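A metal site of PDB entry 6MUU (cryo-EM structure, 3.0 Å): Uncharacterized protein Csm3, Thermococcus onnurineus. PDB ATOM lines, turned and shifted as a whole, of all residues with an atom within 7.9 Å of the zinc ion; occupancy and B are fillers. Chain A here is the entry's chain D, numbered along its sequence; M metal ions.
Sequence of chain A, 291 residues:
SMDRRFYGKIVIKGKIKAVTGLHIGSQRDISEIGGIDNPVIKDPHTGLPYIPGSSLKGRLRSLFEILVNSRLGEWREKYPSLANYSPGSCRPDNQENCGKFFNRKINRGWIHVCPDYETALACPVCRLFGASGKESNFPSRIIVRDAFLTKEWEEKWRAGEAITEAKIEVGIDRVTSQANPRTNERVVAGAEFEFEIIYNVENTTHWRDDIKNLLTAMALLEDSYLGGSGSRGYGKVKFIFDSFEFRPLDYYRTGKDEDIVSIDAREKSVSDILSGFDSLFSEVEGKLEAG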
ATOM      1  N   ARG A  61     -25.013  17.578 -21.428  1.00  0.00           N
ATOM      2  CA  ARG A  61     -24.630  16.185 -21.223  1.00  0.00           C
ATOM      3  C   ARG A  61     -24.553  15.453 -22.552  1.00  0.00           C
ATOM      4  O   ARG A  61     -23.674  14.601 -22.737  1.00  0.00           O
ATOM      5  CB  ARG A  61     -25.607  15.481 -20.290  1.00  0.00           C
ATOM      6  CG  ARG A  61     -25.221  14.039 -19.948  1.00  0.00           C
ATOM      7  CD  ARG A  61     -26.297  13.328 -19.136  1.00  0.00           C
ATOM      8  NE  ARG A  61     -26.086  11.889 -19.070  1.00  0.00           N
ATOM      9  CZ  ARG A  61     -25.561  11.240 -18.026  1.00  0.00           C
ATOM     10  NH1 ARG A  61     -25.249  11.880 -16.930  1.00  0.00           N
ATOM     11  NH2 ARG A  61     -25.403   9.936 -18.078  1.00  0.00           N
ATOM     12  N   PHE A  64     -21.332  16.554 -24.432  1.00  0.00           N
ATOM     13  CA  PHE A  64     -20.121  16.096 -23.770  1.00  0.00           C
ATOM     14  C   PHE A  64     -19.919  14.600 -23.941  1.00  0.00           C
ATOM     15  O   PHE A  64     -18.780  14.123 -23.819  1.00  0.00           O
ATOM     16  CB  PHE A  64     -20.187  16.473 -22.294  1.00  0.00           C
ATOM     17  CG  PHE A  64     -18.920  16.234 -21.557  1.00  0.00           C
ATOM     18  CD1 PHE A  64     -17.820  17.039 -21.781  1.00  0.00           C
ATOM     19  CD2 PHE A  64     -18.836  15.223 -20.627  1.00  0.00           C
ATOM     20  CE1 PHE A  64     -16.654  16.821 -21.098  1.00  0.00           C
ATOM     21  CE2 PHE A  64     -17.668  14.995 -19.941  1.00  0.00           C
ATOM     22  CZ  PHE A  64     -16.579  15.806 -20.173  1.00  0.00           C
ATOM     23  N   GLU A  65     -20.973  13.848 -24.238  1.00  0.00           N
ATOM     24  CA  GLU A  65     -20.844  12.413 -24.460  1.00  0.00           C
ATOM     25  C   GLU A  65     -20.296  12.102 -25.852  1.00  0.00           C
ATOM     26  O   GLU A  65     -19.551  11.131 -26.016  1.00  0.00           O
ATOM     27  CB  GLU A  65     -22.187  11.736 -24.258  1.00  0.00           C
ATOM     28  CG  GLU A  65     -22.574  11.570 -22.815  1.00  0.00           C
ATOM     29  CD  GLU A  65     -24.027  11.234 -22.667  1.00  0.00           C
ATOM     30  OE1 GLU A  65     -24.758  11.363 -23.661  1.00  0.00           O
ATOM     31  OE2 GLU A  65     -24.453  10.832 -21.570  1.00  0.00           O
ATOM     32  N   VAL A  68     -16.621  12.602 -25.779  1.00  0.00           N
ATOM     33  CA  VAL A  68     -15.825  11.530 -25.189  1.00  0.00           C
ATOM     34  C   VAL A  68     -15.551  10.425 -26.206  1.00  0.00           C
ATOM     35  O   VAL A  68     -14.432   9.941 -26.321  1.00  0.00           O
ATOM     36  CB  VAL A  68     -16.522  11.011 -23.920  1.00  0.00           C
ATOM     37  CG1 VAL A  68     -15.898   9.732 -23.431  1.00  0.00           C
ATOM     38  CG2 VAL A  68     -16.419  12.049 -22.838  1.00  0.00           C
ATOM     39  N   PRO A  80     -10.116   6.453 -14.934  1.00  0.00           N
ATOM     40  CA  PRO A  80     -10.419   5.025 -14.955  1.00  0.00           C
ATOM     41  C   PRO A  80     -11.861   4.790 -15.390  1.00  0.00           C
ATOM     42  O   PRO A  80     -12.669   5.705 -15.522  1.00  0.00           O
ATOM     43  CB  PRO A  80     -10.199   4.583 -13.507  1.00  0.00           C
ATOM     44  CG  PRO A  80      -9.280   5.604 -12.953  1.00  0.00           C
ATOM     45  CD  PRO A  80      -9.662   6.895 -13.611  1.00  0.00           C
ATOM     46  N   SER A  81     -12.161   3.511 -15.614  1.00  0.00           N
ATOM     47  CA  SER A  81     -13.467   2.990 -16.019  1.00  0.00           C
ATOM     48  C   SER A  81     -13.965   3.572 -17.335  1.00  0.00           C
ATOM     49  O   SER A  81     -15.168   3.545 -17.616  1.00  0.00           O
ATOM     50  CB  SER A  81     -14.527   3.200 -14.928  1.00  0.00           C
ATOM     51  OG  SER A  81     -14.897   4.567 -14.815  1.00  0.00           O
ATOM     52  N   LEU A  82     -13.065   4.111 -18.158  1.00  0.00           N
ATOM     53  CA  LEU A  82     -13.386   4.368 -19.546  1.00  0.00           C
ATOM     54  C   LEU A  82     -12.876   3.254 -20.449  1.00  0.00           C
ATOM     55  O   LEU A  82     -13.213   3.237 -21.643  1.00  0.00           O
ATOM     56  CB  LEU A  82     -12.800   5.718 -19.991  1.00  0.00           C
ATOM     57  CG  LEU A  82     -13.224   6.954 -19.200  1.00  0.00           C
ATOM     58  CD1 LEU A  82     -12.681   8.215 -19.842  1.00  0.00           C
ATOM     59  CD2 LEU A  82     -14.725   7.030 -18.991  1.00  0.00           C
ATOM     60  N   TYR A  85     -15.441  -0.527 -21.910  1.00  0.00           N
ATOM     61  CA  TYR A  85     -16.351  -0.617 -23.044  1.00  0.00           C
ATOM     62  C   TYR A  85     -15.611  -0.388 -24.354  1.00  0.00           C
ATOM     63  O   TYR A  85     -14.377  -0.334 -24.399  1.00  0.00           O
ATOM     64  CB  TYR A  85     -17.513   0.368 -22.860  1.00  0.00           C
ATOM     65  CG  TYR A  85     -17.063   1.748 -22.504  1.00  0.00           C
ATOM     66  CD1 TYR A  85     -17.049   2.180 -21.185  1.00  0.00           C
ATOM     67  CD2 TYR A  85     -16.591   2.616 -23.485  1.00  0.00           C
ATOM     68  CE1 TYR A  85     -16.612   3.440 -20.862  1.00  0.00           C
ATOM     69  CE2 TYR A  85     -16.138   3.855 -23.174  1.00  0.00           C
ATOM     70  CZ  TYR A  85     -16.154   4.263 -21.871  1.00  0.00           C
ATOM     71  OH  TYR A  85     -15.706   5.534 -21.637  1.00  0.00           O
ATOM     72  N   PHE A 101     -20.317   2.475 -24.976  1.00  0.00           N
ATOM     73  CA  PHE A 101     -20.370   3.685 -24.162  1.00  0.00           C
ATOM     74  C   PHE A 101     -21.815   4.111 -23.915  1.00  0.00           C
ATOM     75  O   PHE A 101     -22.163   4.520 -22.809  1.00  0.00           O
ATOM     76  CB  PHE A 101     -19.582   4.803 -24.838  1.00  0.00           C
ATOM     77  CG  PHE A 101     -19.482   6.067 -24.028  1.00  0.00           C
ATOM     78  CD1 PHE A 101     -18.739   6.093 -22.876  1.00  0.00           C
ATOM     79  CD2 PHE A 101     -20.093   7.228 -24.450  1.00  0.00           C
ATOM     80  CE1 PHE A 101     -18.605   7.239 -22.140  1.00  0.00           C
ATOM     81  CE2 PHE A 101     -19.967   8.384 -23.709  1.00  0.00           C
ATOM     82  CZ  PHE A 101     -19.227   8.387 -22.556  1.00  0.00           C
ATOM     83  N   ASN A 103     -24.746   2.908 -22.980  1.00  0.00           N
ATOM     84  CA  ASN A 103     -25.080   1.617 -22.394  1.00  0.00           C
ATOM     85  C   ASN A 103     -26.516   1.510 -21.900  1.00  0.00           C
ATOM     86  O   ASN A 103     -27.110   0.440 -21.996  1.00  0.00           O
ATOM     87  CB  ASN A 103     -24.094   1.306 -21.270  1.00  0.00           C
ATOM     88  CG  ASN A 103     -23.975   2.431 -20.281  1.00  0.00           C
ATOM     89  OD1 ASN A 103     -24.668   3.441 -20.385  1.00  0.00           O
ATOM     90  ND2 ASN A 103     -23.071   2.290 -19.319  1.00  0.00           N
ATOM     91  N   HIS A 112     -25.494   7.298 -22.404  1.00  0.00           N
ATOM     92  CA  HIS A 112     -24.410   6.858 -21.538  1.00  0.00           C
ATOM     93  C   HIS A 112     -24.722   7.138 -20.078  1.00  0.00           C
ATOM     94  O   HIS A 112     -24.774   8.300 -19.674  1.00  0.00           O
ATOM     95  CB  HIS A 112     -23.094   7.527 -21.899  1.00  0.00           C
ATOM     96  CG  HIS A 112     -22.034   7.251 -20.886  1.00  0.00           C
ATOM     97  ND1 HIS A 112     -21.515   5.993 -20.678  1.00  0.00           N
ATOM     98  CD2 HIS A 112     -21.437   8.060 -19.981  1.00  0.00           C
ATOM     99  CE1 HIS A 112     -20.618   6.047 -19.704  1.00  0.00           C
ATOM    100  NE2 HIS A 112     -20.552   7.295 -19.270  1.00  0.00           N
ATOM    101  N   VAL A 113     -24.912   6.080 -19.304  1.00  0.00           N
ATOM    102  CA  VAL A 113     -25.133   6.155 -17.862  1.00  0.00           C
ATOM    103  C   VAL A 113     -24.331   5.038 -17.205  1.00  0.00           C
ATOM    104  O   VAL A 113     -24.514   3.870 -17.543  1.00  0.00           O
ATOM    105  CB  VAL A 113     -26.623   6.012 -17.482  1.00  0.00           C
ATOM    106  CG1 VAL A 113     -26.737   5.931 -16.017  1.00  0.00           C
ATOM    107  CG2 VAL A 113     -27.458   7.172 -17.986  1.00  0.00           C
ATOM    108  N   CYS A 114     -23.448   5.390 -16.267  1.00  0.00           N
ATOM    109  CA  CYS A 114     -22.731   4.371 -15.519  1.00  0.00           C
ATOM    110  C   CYS A 114     -23.684   3.633 -14.580  1.00  0.00           C
ATOM    111  O   CYS A 114     -24.615   4.215 -14.035  1.00  0.00           O
ATOM    112  CB  CYS A 114     -21.592   4.996 -14.719  1.00  0.00           C
ATOM    113  SG  CYS A 114     -20.276   5.648 -15.765  1.00  0.00           S
ATOM    114  N   PRO A 115     -23.483   2.319 -14.402  1.00  0.00           N
ATOM    115  CA  PRO A 115     -24.461   1.536 -13.640  1.00  0.00           C
ATOM    116  C   PRO A 115     -24.161   1.427 -12.161  1.00  0.00           C
ATOM    117  O   PRO A 115     -25.031   1.015 -11.378  1.00  0.00           O
ATOM    118  CB  PRO A 115     -24.378   0.158 -14.312  1.00  0.00           C
ATOM    119  CG  PRO A 115     -22.963   0.075 -14.730  1.00  0.00           C
ATOM    120  CD  PRO A 115     -22.548   1.459 -15.143  1.00  0.00           C
ATOM    121  N   THR A 119     -17.991   3.052 -10.504  1.00  0.00           N
ATOM    122  CA  THR A 119     -17.617   3.388 -11.865  1.00  0.00           C
ATOM    123  C   THR A 119     -18.102   4.768 -12.287  1.00  0.00           C
ATOM    124  O   THR A 119     -17.633   5.293 -13.298  1.00  0.00           O
ATOM    125  CB  THR A 119     -18.123   2.337 -12.844  1.00  0.00           C
ATOM    126  OG1 THR A 119     -17.674   2.651 -14.167  1.00  0.00           O
ATOM    127  CG2 THR A 119     -19.631   2.266 -12.849  1.00  0.00           C
ATOM    128  N   ALA A 120     -19.034   5.353 -11.530  1.00  0.00           N
ATOM    129  CA  ALA A 120     -19.487   6.714 -11.824  1.00  0.00           C
ATOM    130  C   ALA A 120     -18.616   7.769 -11.173  1.00  0.00           C
ATOM    131  O   ALA A 120     -18.676   8.932 -11.581  1.00  0.00           O
ATOM    132  CB  ALA A 120     -20.934   6.896 -11.365  1.00  0.00           C
ATOM    133  N   LEU A 121     -17.836   7.401 -10.162  1.00  0.00           N
ATOM    134  CA  LEU A 121     -16.920   8.324  -9.529  1.00  0.00           C
ATOM    135  C   LEU A 121     -15.627   8.470 -10.318  1.00  0.00           C
ATOM    136  O   LEU A 121     -14.842   9.376 -10.039  1.00  0.00           O
ATOM    137  CB  LEU A 121     -16.654   7.858  -8.098  1.00  0.00           C
ATOM    138  CG  LEU A 121     -16.049   8.751  -7.018  1.00  0.00           C
ATOM    139  CD1 LEU A 121     -16.669   8.371  -5.713  1.00  0.00           C
ATOM    140  CD2 LEU A 121     -14.546   8.617  -6.889  1.00  0.00           C
ATOM    141  N   ALA A 122     -15.409   7.624 -11.310  1.00  0.00           N
ATOM    142  CA  ALA A 122     -14.250   7.730 -12.179  1.00  0.00           C
ATOM    143  C   ALA A 122     -14.569   8.257 -13.567  1.00  0.00           C
ATOM    144  O   ALA A 122     -13.668   8.786 -14.235  1.00  0.00           O
ATOM    145  CB  ALA A 122     -13.556   6.365 -12.314  1.00  0.00           C
ATOM    146  N   CYS A 123     -15.816   8.152 -14.010  1.00  0.00           N
ATOM    147  CA  CYS A 123     -16.190   8.637 -15.334  1.00  0.00           C
ATOM    148  C   CYS A 123     -16.292  10.164 -15.316  1.00  0.00           C
ATOM    149  O   CYS A 123     -16.873  10.723 -14.395  1.00  0.00           O
ATOM    150  CB  CYS A 123     -17.518   8.037 -15.770  1.00  0.00           C
ATOM    151  SG  CYS A 123     -18.083   8.581 -17.385  1.00  0.00           S
ATOM    152  N   PRO A 124     -15.745  10.850 -16.328  1.00  0.00           N
ATOM    153  CA  PRO A 124     -15.897  12.305 -16.359  1.00  0.00           C
ATOM    154  C   PRO A 124     -17.310  12.758 -16.674  1.00  0.00           C
ATOM    155  O   PRO A 124     -17.706  13.849 -16.243  1.00  0.00           O
ATOM    156  CB  PRO A 124     -14.916  12.739 -17.453  1.00  0.00           C
ATOM    157  CG  PRO A 124     -14.823  11.564 -18.339  1.00  0.00           C
ATOM    158  CD  PRO A 124     -14.924  10.362 -17.437  1.00  0.00           C
ATOM    159  N   VAL A 125     -18.067  11.957 -17.419  1.00  0.00           N
ATOM    160  CA  VAL A 125     -19.444  12.325 -17.728  1.00  0.00           C
ATOM    161  C   VAL A 125     -20.310  12.181 -16.481  1.00  0.00           C
ATOM    162  O   VAL A 125     -21.162  13.023 -16.207  1.00  0.00           O
ATOM    163  CB  VAL A 125     -19.970  11.475 -18.892  1.00  0.00           C
ATOM    164  CG1 VAL A 125     -21.380  11.850 -19.257  1.00  0.00           C
ATOM    165  CG2 VAL A 125     -19.059  11.614 -20.085  1.00  0.00           C
ATOM    166  N   CYS A 126     -20.093  11.137 -15.690  1.00  0.00           N
ATOM    167  CA  CYS A 126     -21.008  10.839 -14.602  1.00  0.00           C
ATOM    168  C   CYS A 126     -20.567  11.351 -13.246  1.00  0.00           C
ATOM    169  O   CYS A 126     -21.365  11.261 -12.306  1.00  0.00           O
ATOM    170  CB  CYS A 126     -21.278   9.336 -14.536  1.00  0.00           C
ATOM    171  SG  CYS A 126     -22.214   8.721 -15.945  1.00  0.00           S
ATOM    172  N   ARG A 127     -19.356  11.883 -13.091  1.00  0.00           N
ATOM    173  CA  ARG A 127     -19.094  12.657 -11.884  1.00  0.00           C
ATOM    174  C   ARG A 127     -19.840  13.972 -11.920  1.00  0.00           C
ATOM    175  O   ARG A 127     -20.429  14.389 -10.919  1.00  0.00           O
ATOM    176  CB  ARG A 127     -17.607  12.954 -11.700  1.00  0.00           C
ATOM    177  CG  ARG A 127     -16.700  11.819 -11.378  1.00  0.00           C
ATOM    178  CD  ARG A 127     -15.317  12.390 -11.225  1.00  0.00           C
ATOM    179  NE  ARG A 127     -15.023  13.249 -12.364  1.00  0.00           N
ATOM    180  CZ  ARG A 127     -13.904  13.922 -12.541  1.00  0.00           C
ATOM    181  NH1 ARG A 127     -12.911  13.813 -11.669  1.00  0.00           N
ATOM    182  NH2 ARG A 127     -13.756  14.696 -13.599  1.00  0.00           N
ATOM    183  N   LEU A 128     -19.812  14.646 -13.056  1.00  0.00           N
ATOM    184  CA  LEU A 128     -20.352  15.985 -13.142  1.00  0.00           C
ATOM    185  C   LEU A 128     -21.874  15.977 -13.257  1.00  0.00           C
ATOM    186  O   LEU A 128     -22.524  16.932 -12.820  1.00  0.00           O
ATOM    187  CB  LEU A 128     -19.721  16.698 -14.341  1.00  0.00           C
ATOM    188  CG  LEU A 128     -19.738  18.202 -14.492  1.00  0.00           C
ATOM    189  CD1 LEU A 128     -18.525  18.551 -15.279  1.00  0.00           C
ATOM    190  CD2 LEU A 128     -20.941  18.694 -15.236  1.00  0.00           C
ATOM    191  N   GLY A 130     -24.015  12.837 -12.794  1.00  0.00           N
ATOM    192  CA  GLY A 130     -24.702  11.839 -11.983  1.00  0.00           C
ATOM    193  C   GLY A 130     -25.101  10.603 -12.770  1.00  0.00           C
ATOM    194  O   GLY A 130     -25.148  10.596 -13.997  1.00  0.00           O
ATOM    195  N   ALA A 131     -25.394   9.525 -12.036  1.00  0.00           N
ATOM    196  CA  ALA A 131     -25.600   8.232 -12.685  1.00  0.00           C
ATOM    197  C   ALA A 131     -27.003   7.647 -12.517  1.00  0.00           C
ATOM    198  O   ALA A 131     -27.718   7.567 -13.505  1.00  0.00           O
ATOM    199  CB  ALA A 131     -24.556   7.246 -12.160  1.00  0.00           C
HETATM  200 ZN    ZN M   1     -19.853   8.133 -17.036  1.00  0.00          ZN
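SG of Cys 123 lies close to N of Val 125.
The backbone carbonyl oxygen of Phe 101 lies within hydrogen-bond range of a ring nitrogen (ND1) of His 112 (2.7 Å).
The side-chain sulfur (SG) of Cys 126 lies close to the backbone NH (N) of Cys 114, at 3.6 Å.
The side-chain sulfur (SG) of Cys 114 sits at hydrogen-bond distance from the backbone carbonyl oxygen (O) of Thr 119 (3.6 Å).
Residues that only touch the zinc ion: Val 125 (3.8 Å).
The nearest printed residue that does not touch the zinc ion is Pro 124 (5.0 Å).
The zinc ion is bound by the side-chain sulfur of Cys 123 (1.9 Å), a ring nitrogen (NE2) of His 112 (2.5 Å) and the side-chain sulfur of Cys 126 (2.7 Å).
Slightly farther from the zinc ion lies SG of Cys 114 (2.8 Å).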
